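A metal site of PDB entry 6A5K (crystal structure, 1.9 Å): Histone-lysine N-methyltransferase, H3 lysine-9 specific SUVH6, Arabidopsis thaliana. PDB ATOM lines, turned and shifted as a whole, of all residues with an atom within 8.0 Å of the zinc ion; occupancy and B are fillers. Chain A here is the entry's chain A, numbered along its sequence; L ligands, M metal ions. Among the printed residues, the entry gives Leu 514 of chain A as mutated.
The zinc ion is bound by SG of Cys 522, 2.3 Å away.
The zinc ion is bound by the side-chain sulfur (SG) of Cys 517, at 2.4 Å.
The zinc ion is bound by SG of Cys 515 (2.4 Å).
The zinc ion is bound by the side-chain sulfur (SG) of Cys 457, at 2.4 Å.
The zinc ion has four donor atoms within binding distance.
The side-chain sulfur of Cys 515 lies close to a nitrogen (N4) of the ligand.
O of His 455 sits at hydrogen-bond distance from N4 of the ligand (3.0 Å).
O of Arg 363 is in hydrogen-bond range of N1 of the ligand.
A nitrogen (N3) of the ligand lies within hydrogen-bond range of the backbone NH (N) of His 455, at 3.0 Å.
A nitrogen (N5) of the ligand lies within hydrogen-bond range of the backbone NH (N) of Phe 516 (2.8 Å).
The side-chain sulfur of Cys 517 lies close to the backbone NH of Ala 519 (3.4 Å).
N of Cys 515 sits at hydrogen-bond distance from O of Arg 524 (2.9 Å).
SG of Cys 522 sits close to N of Arg 524, at 3.2 Å.
A ring nitrogen (NE2) of His 455 sits close to the side-chain sulfur of Cys 457, at 3.4 Å.
The guanidinium group of Arg 523 lies within hydrogen-bond range of the backbone carbonyl oxygen of Cys 457, at 3.5 Å.
Along chain A the residues within 4 Å of the zinc ion span positions 457 to 522.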
ATOM      1  N   ARG A 363     -11.406 -10.923 -14.299  1.00  0.00           N
ATOM      2  CA  ARG A 363     -11.727 -10.496 -12.935  1.00  0.00           C
ATOM      3  C   ARG A 363     -13.110  -9.843 -12.834  1.00  0.00           C
ATOM      4  O   ARG A 363     -13.350  -9.043 -11.937  1.00  0.00           O
ATOM      5  CB  ARG A 363     -10.658  -9.518 -12.421  1.00  0.00           C
ATOM      6  CG  ARG A 363      -9.309 -10.180 -12.195  1.00  0.00           C
ATOM      7  CD  ARG A 363      -8.203  -9.151 -11.873  1.00  0.00           C
ATOM      8  NE  ARG A 363      -8.236  -8.010 -12.789  1.00  0.00           N
ATOM      9  CZ  ARG A 363      -7.900  -8.051 -14.072  1.00  0.00           C
ATOM     10  NH1 ARG A 363      -7.479  -9.187 -14.605  1.00  0.00           N
ATOM     11  NH2 ARG A 363      -7.994  -6.960 -14.823  1.00  0.00           N
ATOM     12  N   HIS A 455      -8.732  -6.188  -6.820  1.00  0.00           N
ATOM     13  CA  HIS A 455      -7.444  -6.259  -6.133  1.00  0.00           C
ATOM     14  C   HIS A 455      -6.271  -6.232  -7.115  1.00  0.00           C
ATOM     15  O   HIS A 455      -6.357  -6.802  -8.207  1.00  0.00           O
ATOM     16  CB  HIS A 455      -7.342  -7.536  -5.291  1.00  0.00           C
ATOM     17  CG  HIS A 455      -5.929  -7.882  -4.923  1.00  0.00           C
ATOM     18  ND1 HIS A 455      -5.302  -7.338  -3.828  1.00  0.00           N
ATOM     19  CD2 HIS A 455      -5.019  -8.684  -5.532  1.00  0.00           C
ATOM     20  CE1 HIS A 455      -4.057  -7.803  -3.753  1.00  0.00           C
ATOM     21  NE2 HIS A 455      -3.867  -8.621  -4.780  1.00  0.00           N
ATOM     22  N   SER A 456      -5.185  -5.596  -6.702  1.00  0.00           N
ATOM     23  CA  SER A 456      -3.920  -5.760  -7.409  1.00  0.00           C
ATOM     24  C   SER A 456      -2.740  -5.872  -6.439  1.00  0.00           C
ATOM     25  O   SER A 456      -2.734  -5.237  -5.379  1.00  0.00           O
ATOM     26  CB  SER A 456      -3.671  -4.598  -8.375  1.00  0.00           C
ATOM     27  OG  SER A 456      -2.428  -4.762  -9.053  1.00  0.00           O
ATOM     28  N   CYS A 457      -1.757  -6.675  -6.815  1.00  0.00           N
ATOM     29  CA  CYS A 457      -0.529  -6.801  -6.035  1.00  0.00           C
ATOM     30  C   CYS A 457       0.399  -5.623  -6.315  1.00  0.00           C
ATOM     31  O   CYS A 457       1.385  -5.415  -5.612  1.00  0.00           O
ATOM     32  CB  CYS A 457       0.169  -8.118  -6.332  1.00  0.00           C
ATOM     33  SG  CYS A 457      -0.841  -9.568  -5.935  1.00  0.00           S
ATOM     34  N   SER A 458       0.091  -4.868  -7.361  1.00  0.00           N
ATOM     35  CA  SER A 458       0.773  -3.607  -7.618  1.00  0.00           C
ATOM     36  C   SER A 458      -0.253  -2.503  -7.852  1.00  0.00           C
ATOM     37  O   SER A 458      -0.377  -1.975  -8.959  1.00  0.00           O
ATOM     38  CB  SER A 458       1.715  -3.728  -8.819  1.00  0.00           C
ATOM     39  OG  SER A 458       2.526  -2.580  -8.927  1.00  0.00           O
ATOM     40  N   LEU A 514      -6.921 -18.011  -7.135  1.00  0.00           N
ATOM     41  CA  LEU A 514      -5.748 -17.428  -7.763  1.00  0.00           C
ATOM     42  C   LEU A 514      -5.930 -15.929  -7.967  1.00  0.00           C
ATOM     43  O   LEU A 514      -7.045 -15.460  -8.204  1.00  0.00           O
ATOM     44  CB  LEU A 514      -5.462 -18.115  -9.103  1.00  0.00           C
ATOM     45  CG  LEU A 514      -5.082 -19.588  -9.068  1.00  0.00           C
ATOM     46  CD1 LEU A 514      -5.064 -20.194 -10.483  1.00  0.00           C
ATOM     47  CD2 LEU A 514      -3.723 -19.775  -8.409  1.00  0.00           C
ATOM     48  N   CYS A 515      -4.843 -15.176  -7.867  1.00  0.00           N
ATOM     49  CA  CYS A 515      -4.859 -13.765  -8.210  1.00  0.00           C
ATOM     50  C   CYS A 515      -4.594 -13.589  -9.699  1.00  0.00           C
ATOM     51  O   CYS A 515      -3.614 -14.130 -10.222  1.00  0.00           O
ATOM     52  CB  CYS A 515      -3.824 -12.972  -7.389  1.00  0.00           C
ATOM     53  SG  CYS A 515      -3.857 -11.202  -7.742  1.00  0.00           S
ATOM     54  N   PHE A 516      -5.458 -12.836 -10.370  1.00  0.00           N
ATOM     55  CA  PHE A 516      -5.326 -12.575 -11.800  1.00  0.00           C
ATOM     56  C   PHE A 516      -4.972 -11.114 -12.084  1.00  0.00           C
ATOM     57  O   PHE A 516      -5.310 -10.585 -13.147  1.00  0.00           O
ATOM     58  CB  PHE A 516      -6.629 -12.933 -12.522  1.00  0.00           C
ATOM     59  CG  PHE A 516      -6.899 -14.416 -12.590  1.00  0.00           C
ATOM     60  CD1 PHE A 516      -5.877 -15.341 -12.445  1.00  0.00           C
ATOM     61  CD2 PHE A 516      -8.193 -14.883 -12.811  1.00  0.00           C
ATOM     62  CE1 PHE A 516      -6.124 -16.695 -12.518  1.00  0.00           C
ATOM     63  CE2 PHE A 516      -8.448 -16.241 -12.884  1.00  0.00           C
ATOM     64  CZ  PHE A 516      -7.410 -17.154 -12.730  1.00  0.00           C
ATOM     65  N   CYS A 517      -4.292 -10.459 -11.143  1.00  0.00           N
ATOM     66  CA  CYS A 517      -4.013  -9.024 -11.303  1.00  0.00           C
ATOM     67  C   CYS A 517      -3.028  -8.770 -12.458  1.00  0.00           C
ATOM     68  O   CYS A 517      -3.042  -7.696 -13.054  1.00  0.00           O
ATOM     69  CB  CYS A 517      -3.461  -8.413  -9.997  1.00  0.00           C
ATOM     70  SG  CYS A 517      -1.694  -8.724  -9.620  1.00  0.00           S
ATOM     71  N   GLY A 518      -2.193  -9.763 -12.752  1.00  0.00           N
ATOM     72  CA  GLY A 518      -1.277  -9.679 -13.884  1.00  0.00           C
ATOM     73  C   GLY A 518       0.018  -8.909 -13.654  1.00  0.00           C
ATOM     74  O   GLY A 518       0.817  -8.723 -14.581  1.00  0.00           O
ATOM     75  N   ALA A 519       0.238  -8.464 -12.418  1.00  0.00           N
ATOM     76  CA  ALA A 519       1.471  -7.767 -12.077  1.00  0.00           C
ATOM     77  C   ALA A 519       2.663  -8.721 -12.110  1.00  0.00           C
ATOM     78  O   ALA A 519       2.532  -9.918 -11.878  1.00  0.00           O
ATOM     79  CB  ALA A 519       1.359  -7.110 -10.713  1.00  0.00           C
ATOM     80  N   ALA A 520       3.845  -8.187 -12.393  1.00  0.00           N
ATOM     81  CA  ALA A 520       5.018  -9.062 -12.443  1.00  0.00           C
ATOM     82  C   ALA A 520       5.431  -9.529 -11.049  1.00  0.00           C
ATOM     83  O   ALA A 520       6.074 -10.569 -10.901  1.00  0.00           O
ATOM     84  CB  ALA A 520       6.129  -8.362 -13.117  1.00  0.00           C
ATOM     85  N   VAL A 521       5.049  -8.776 -10.019  1.00  0.00           N
ATOM     86  CA  VAL A 521       5.361  -9.156  -8.636  1.00  0.00           C
ATOM     87  C   VAL A 521       4.156  -9.784  -7.924  1.00  0.00           C
ATOM     88  O   VAL A 521       4.063  -9.779  -6.690  1.00  0.00           O
ATOM     89  CB  VAL A 521       5.850  -7.941  -7.837  1.00  0.00           C
ATOM     90  CG1 VAL A 521       7.024  -7.296  -8.527  1.00  0.00           C
ATOM     91  CG2 VAL A 521       4.698  -6.928  -7.648  1.00  0.00           C
ATOM     92  N   CYS A 522       3.233 -10.334  -8.700  1.00  0.00           N
ATOM     93  CA  CYS A 522       2.013 -10.940  -8.156  1.00  0.00           C
ATOM     94  C   CYS A 522       2.288 -11.999  -7.082  1.00  0.00           C
ATOM     95  O   CYS A 522       3.179 -12.833  -7.229  1.00  0.00           O
ATOM     96  CB  CYS A 522       1.194 -11.551  -9.289  1.00  0.00           C
ATOM     97  SG  CYS A 522      -0.385 -12.269  -8.794  1.00  0.00           S
ATOM     98  N   ARG A 523       1.519 -11.954  -6.001  1.00  0.00           N
ATOM     99  CA  ARG A 523       1.662 -12.911  -4.915  1.00  0.00           C
ATOM    100  C   ARG A 523       0.822 -14.169  -5.169  1.00  0.00           C
ATOM    101  O   ARG A 523       0.722 -15.056  -4.310  1.00  0.00           O
ATOM    102  CB  ARG A 523       1.306 -12.221  -3.597  1.00  0.00           C
ATOM    103  CG  ARG A 523       2.143 -10.938  -3.426  1.00  0.00           C
ATOM    104  CD  ARG A 523       2.082 -10.315  -2.033  1.00  0.00           C
ATOM    105  NE  ARG A 523       0.878  -9.525  -1.823  1.00  0.00           N
ATOM    106  CZ  ARG A 523       0.692  -8.290  -2.294  1.00  0.00           C
ATOM    107  NH1 ARG A 523       1.627  -7.684  -3.006  1.00  0.00           N
ATOM    108  NH2 ARG A 523      -0.450  -7.662  -2.034  1.00  0.00           N
ATOM    109  N   ARG A 524       0.228 -14.216  -6.352  1.00  0.00           N
ATOM    110  CA  ARG A 524      -0.310 -15.441  -6.986  1.00  0.00           C
ATOM    111  C   ARG A 524      -1.646 -15.929  -6.443  1.00  0.00           C
ATOM    112  O   ARG A 524      -2.428 -16.533  -7.181  1.00  0.00           O
ATOM    113  CB  ARG A 524       0.719 -16.577  -6.900  1.00  0.00           C
ATOM    114  CG  ARG A 524       2.033 -16.313  -7.618  1.00  0.00           C
ATOM    115  CD  ARG A 524       1.836 -15.720  -9.010  1.00  0.00           C
ATOM    116  NE  ARG A 524       1.097 -16.608  -9.917  1.00  0.00           N
ATOM    117  CZ  ARG A 524       1.640 -17.657 -10.543  1.00  0.00           C
ATOM    118  NH1 ARG A 524       2.913 -17.957 -10.358  1.00  0.00           N
ATOM    119  NH2 ARG A 524       0.895 -18.400 -11.348  1.00  0.00           N
ATOM    120  N   ARG A 525      -1.917 -15.687  -5.161  1.00  0.00           N
ATOM    121  CA  ARG A 525      -3.203 -16.077  -4.590  1.00  0.00           C
ATOM    122  C   ARG A 525      -3.962 -14.874  -4.043  1.00  0.00           C
ATOM    123  O   ARG A 525      -3.362 -14.009  -3.404  1.00  0.00           O
ATOM    124  CB  ARG A 525      -3.007 -17.113  -3.471  1.00  0.00           C
ATOM    125  CG  ARG A 525      -2.902 -18.552  -3.985  1.00  0.00           C
ATOM    126  CD  ARG A 525      -2.731 -19.561  -2.857  1.00  0.00           C
ATOM    127  NE  ARG A 525      -3.893 -19.612  -1.983  1.00  0.00           N
ATOM    128  CZ  ARG A 525      -3.953 -20.328  -0.865  1.00  0.00           C
ATOM    129  NH1 ARG A 525      -2.916 -21.057  -0.484  1.00  0.00           N
ATOM    130  NH2 ARG A 525      -5.051 -20.312  -0.119  1.00  0.00           N
ATOM    131  N   LEU A 526      -5.257 -14.819  -4.334  1.00  0.00           N
ATOM    132  CA  LEU A 526      -6.113 -13.775  -3.762  1.00  0.00           C
ATOM    133  C   LEU A 526      -6.416 -14.139  -2.304  1.00  0.00           C
ATOM    134  O   LEU A 526      -6.431 -13.275  -1.425  1.00  0.00           O
ATOM    135  CB  LEU A 526      -7.404 -13.637  -4.576  1.00  0.00           C
ATOM    136  CG  LEU A 526      -8.297 -12.424  -4.285  1.00  0.00           C
ATOM    137  CD1 LEU A 526      -7.571 -11.116  -4.572  1.00  0.00           C
ATOM    138  CD2 LEU A 526      -9.585 -12.509  -5.092  1.00  0.00           C
HETATM  139  N1  LIG L   1     -14.895  -8.101 -10.003  1.00  0.00           N
HETATM  140  C1  LIG L   1     -16.012  -7.868  -9.074  1.00  0.00           C
HETATM  141  C2  LIG L   1     -17.383  -7.897  -9.752  1.00  0.00           C
HETATM  142  O1  LIG L   1     -18.400  -7.584  -9.120  1.00  0.00           O
HETATM  143  O2  LIG L   1     -17.497  -8.219 -10.937  1.00  0.00           O
HETATM  144  C3  LIG L   1     -15.831  -6.538  -8.336  1.00  0.00           C
HETATM  145  C4  LIG L   1     -14.826  -6.678  -7.203  1.00  0.00           C
HETATM  146  S1  LIG L   1     -15.556  -7.746  -5.933  1.00  0.00           S
HETATM  147  C5  LIG L   1     -15.428  -6.640  -4.538  1.00  0.00           C
HETATM  148  C6  LIG L   1     -14.239  -8.884  -5.477  1.00  0.00           C
HETATM  149  C7  LIG L   1     -14.218 -10.087  -6.406  1.00  0.00           C
HETATM  150  O3  LIG L   1     -13.645  -9.716  -7.658  1.00  0.00           O
HETATM  151  C8  LIG L   1     -13.353 -11.194  -5.845  1.00  0.00           C
HETATM  152  O4  LIG L   1     -14.102 -12.069  -5.031  1.00  0.00           O
HETATM  153  C9  LIG L   1     -12.888 -11.877  -7.107  1.00  0.00           C
HETATM  154  O5  LIG L   1     -13.929 -12.711  -7.567  1.00  0.00           O
HETATM  155  C10 LIG L   1     -12.768 -10.729  -8.088  1.00  0.00           C
HETATM  156  N2  LIG L   1     -11.384 -10.204  -8.085  1.00  0.00           N
HETATM  157  C11 LIG L   1     -10.960  -8.964  -7.685  1.00  0.00           C
HETATM  158  N3  LIG L   1      -9.615  -8.893  -7.840  1.00  0.00           N
HETATM  159  C12 LIG L   1      -9.164 -10.084  -8.308  1.00  0.00           C
HETATM  160  C13 LIG L   1      -7.910 -10.561  -8.641  1.00  0.00           C
HETATM  161  N4  LIG L   1      -6.819  -9.791  -8.504  1.00  0.00           N
HETATM  162  N5  LIG L   1      -7.770 -11.849  -9.092  1.00  0.00           N
HETATM  163  C14 LIG L   1      -8.880 -12.668  -9.238  1.00  0.00           C
HETATM  164  N6  LIG L   1     -10.138 -12.185  -8.918  1.00  0.00           N
HETATM  165  C15 LIG L   1     -10.281 -10.914  -8.472  1.00  0.00           C
HETATM  166 ZN    ZN M   1      -1.623 -10.481  -8.037  1.00  0.00          ZN
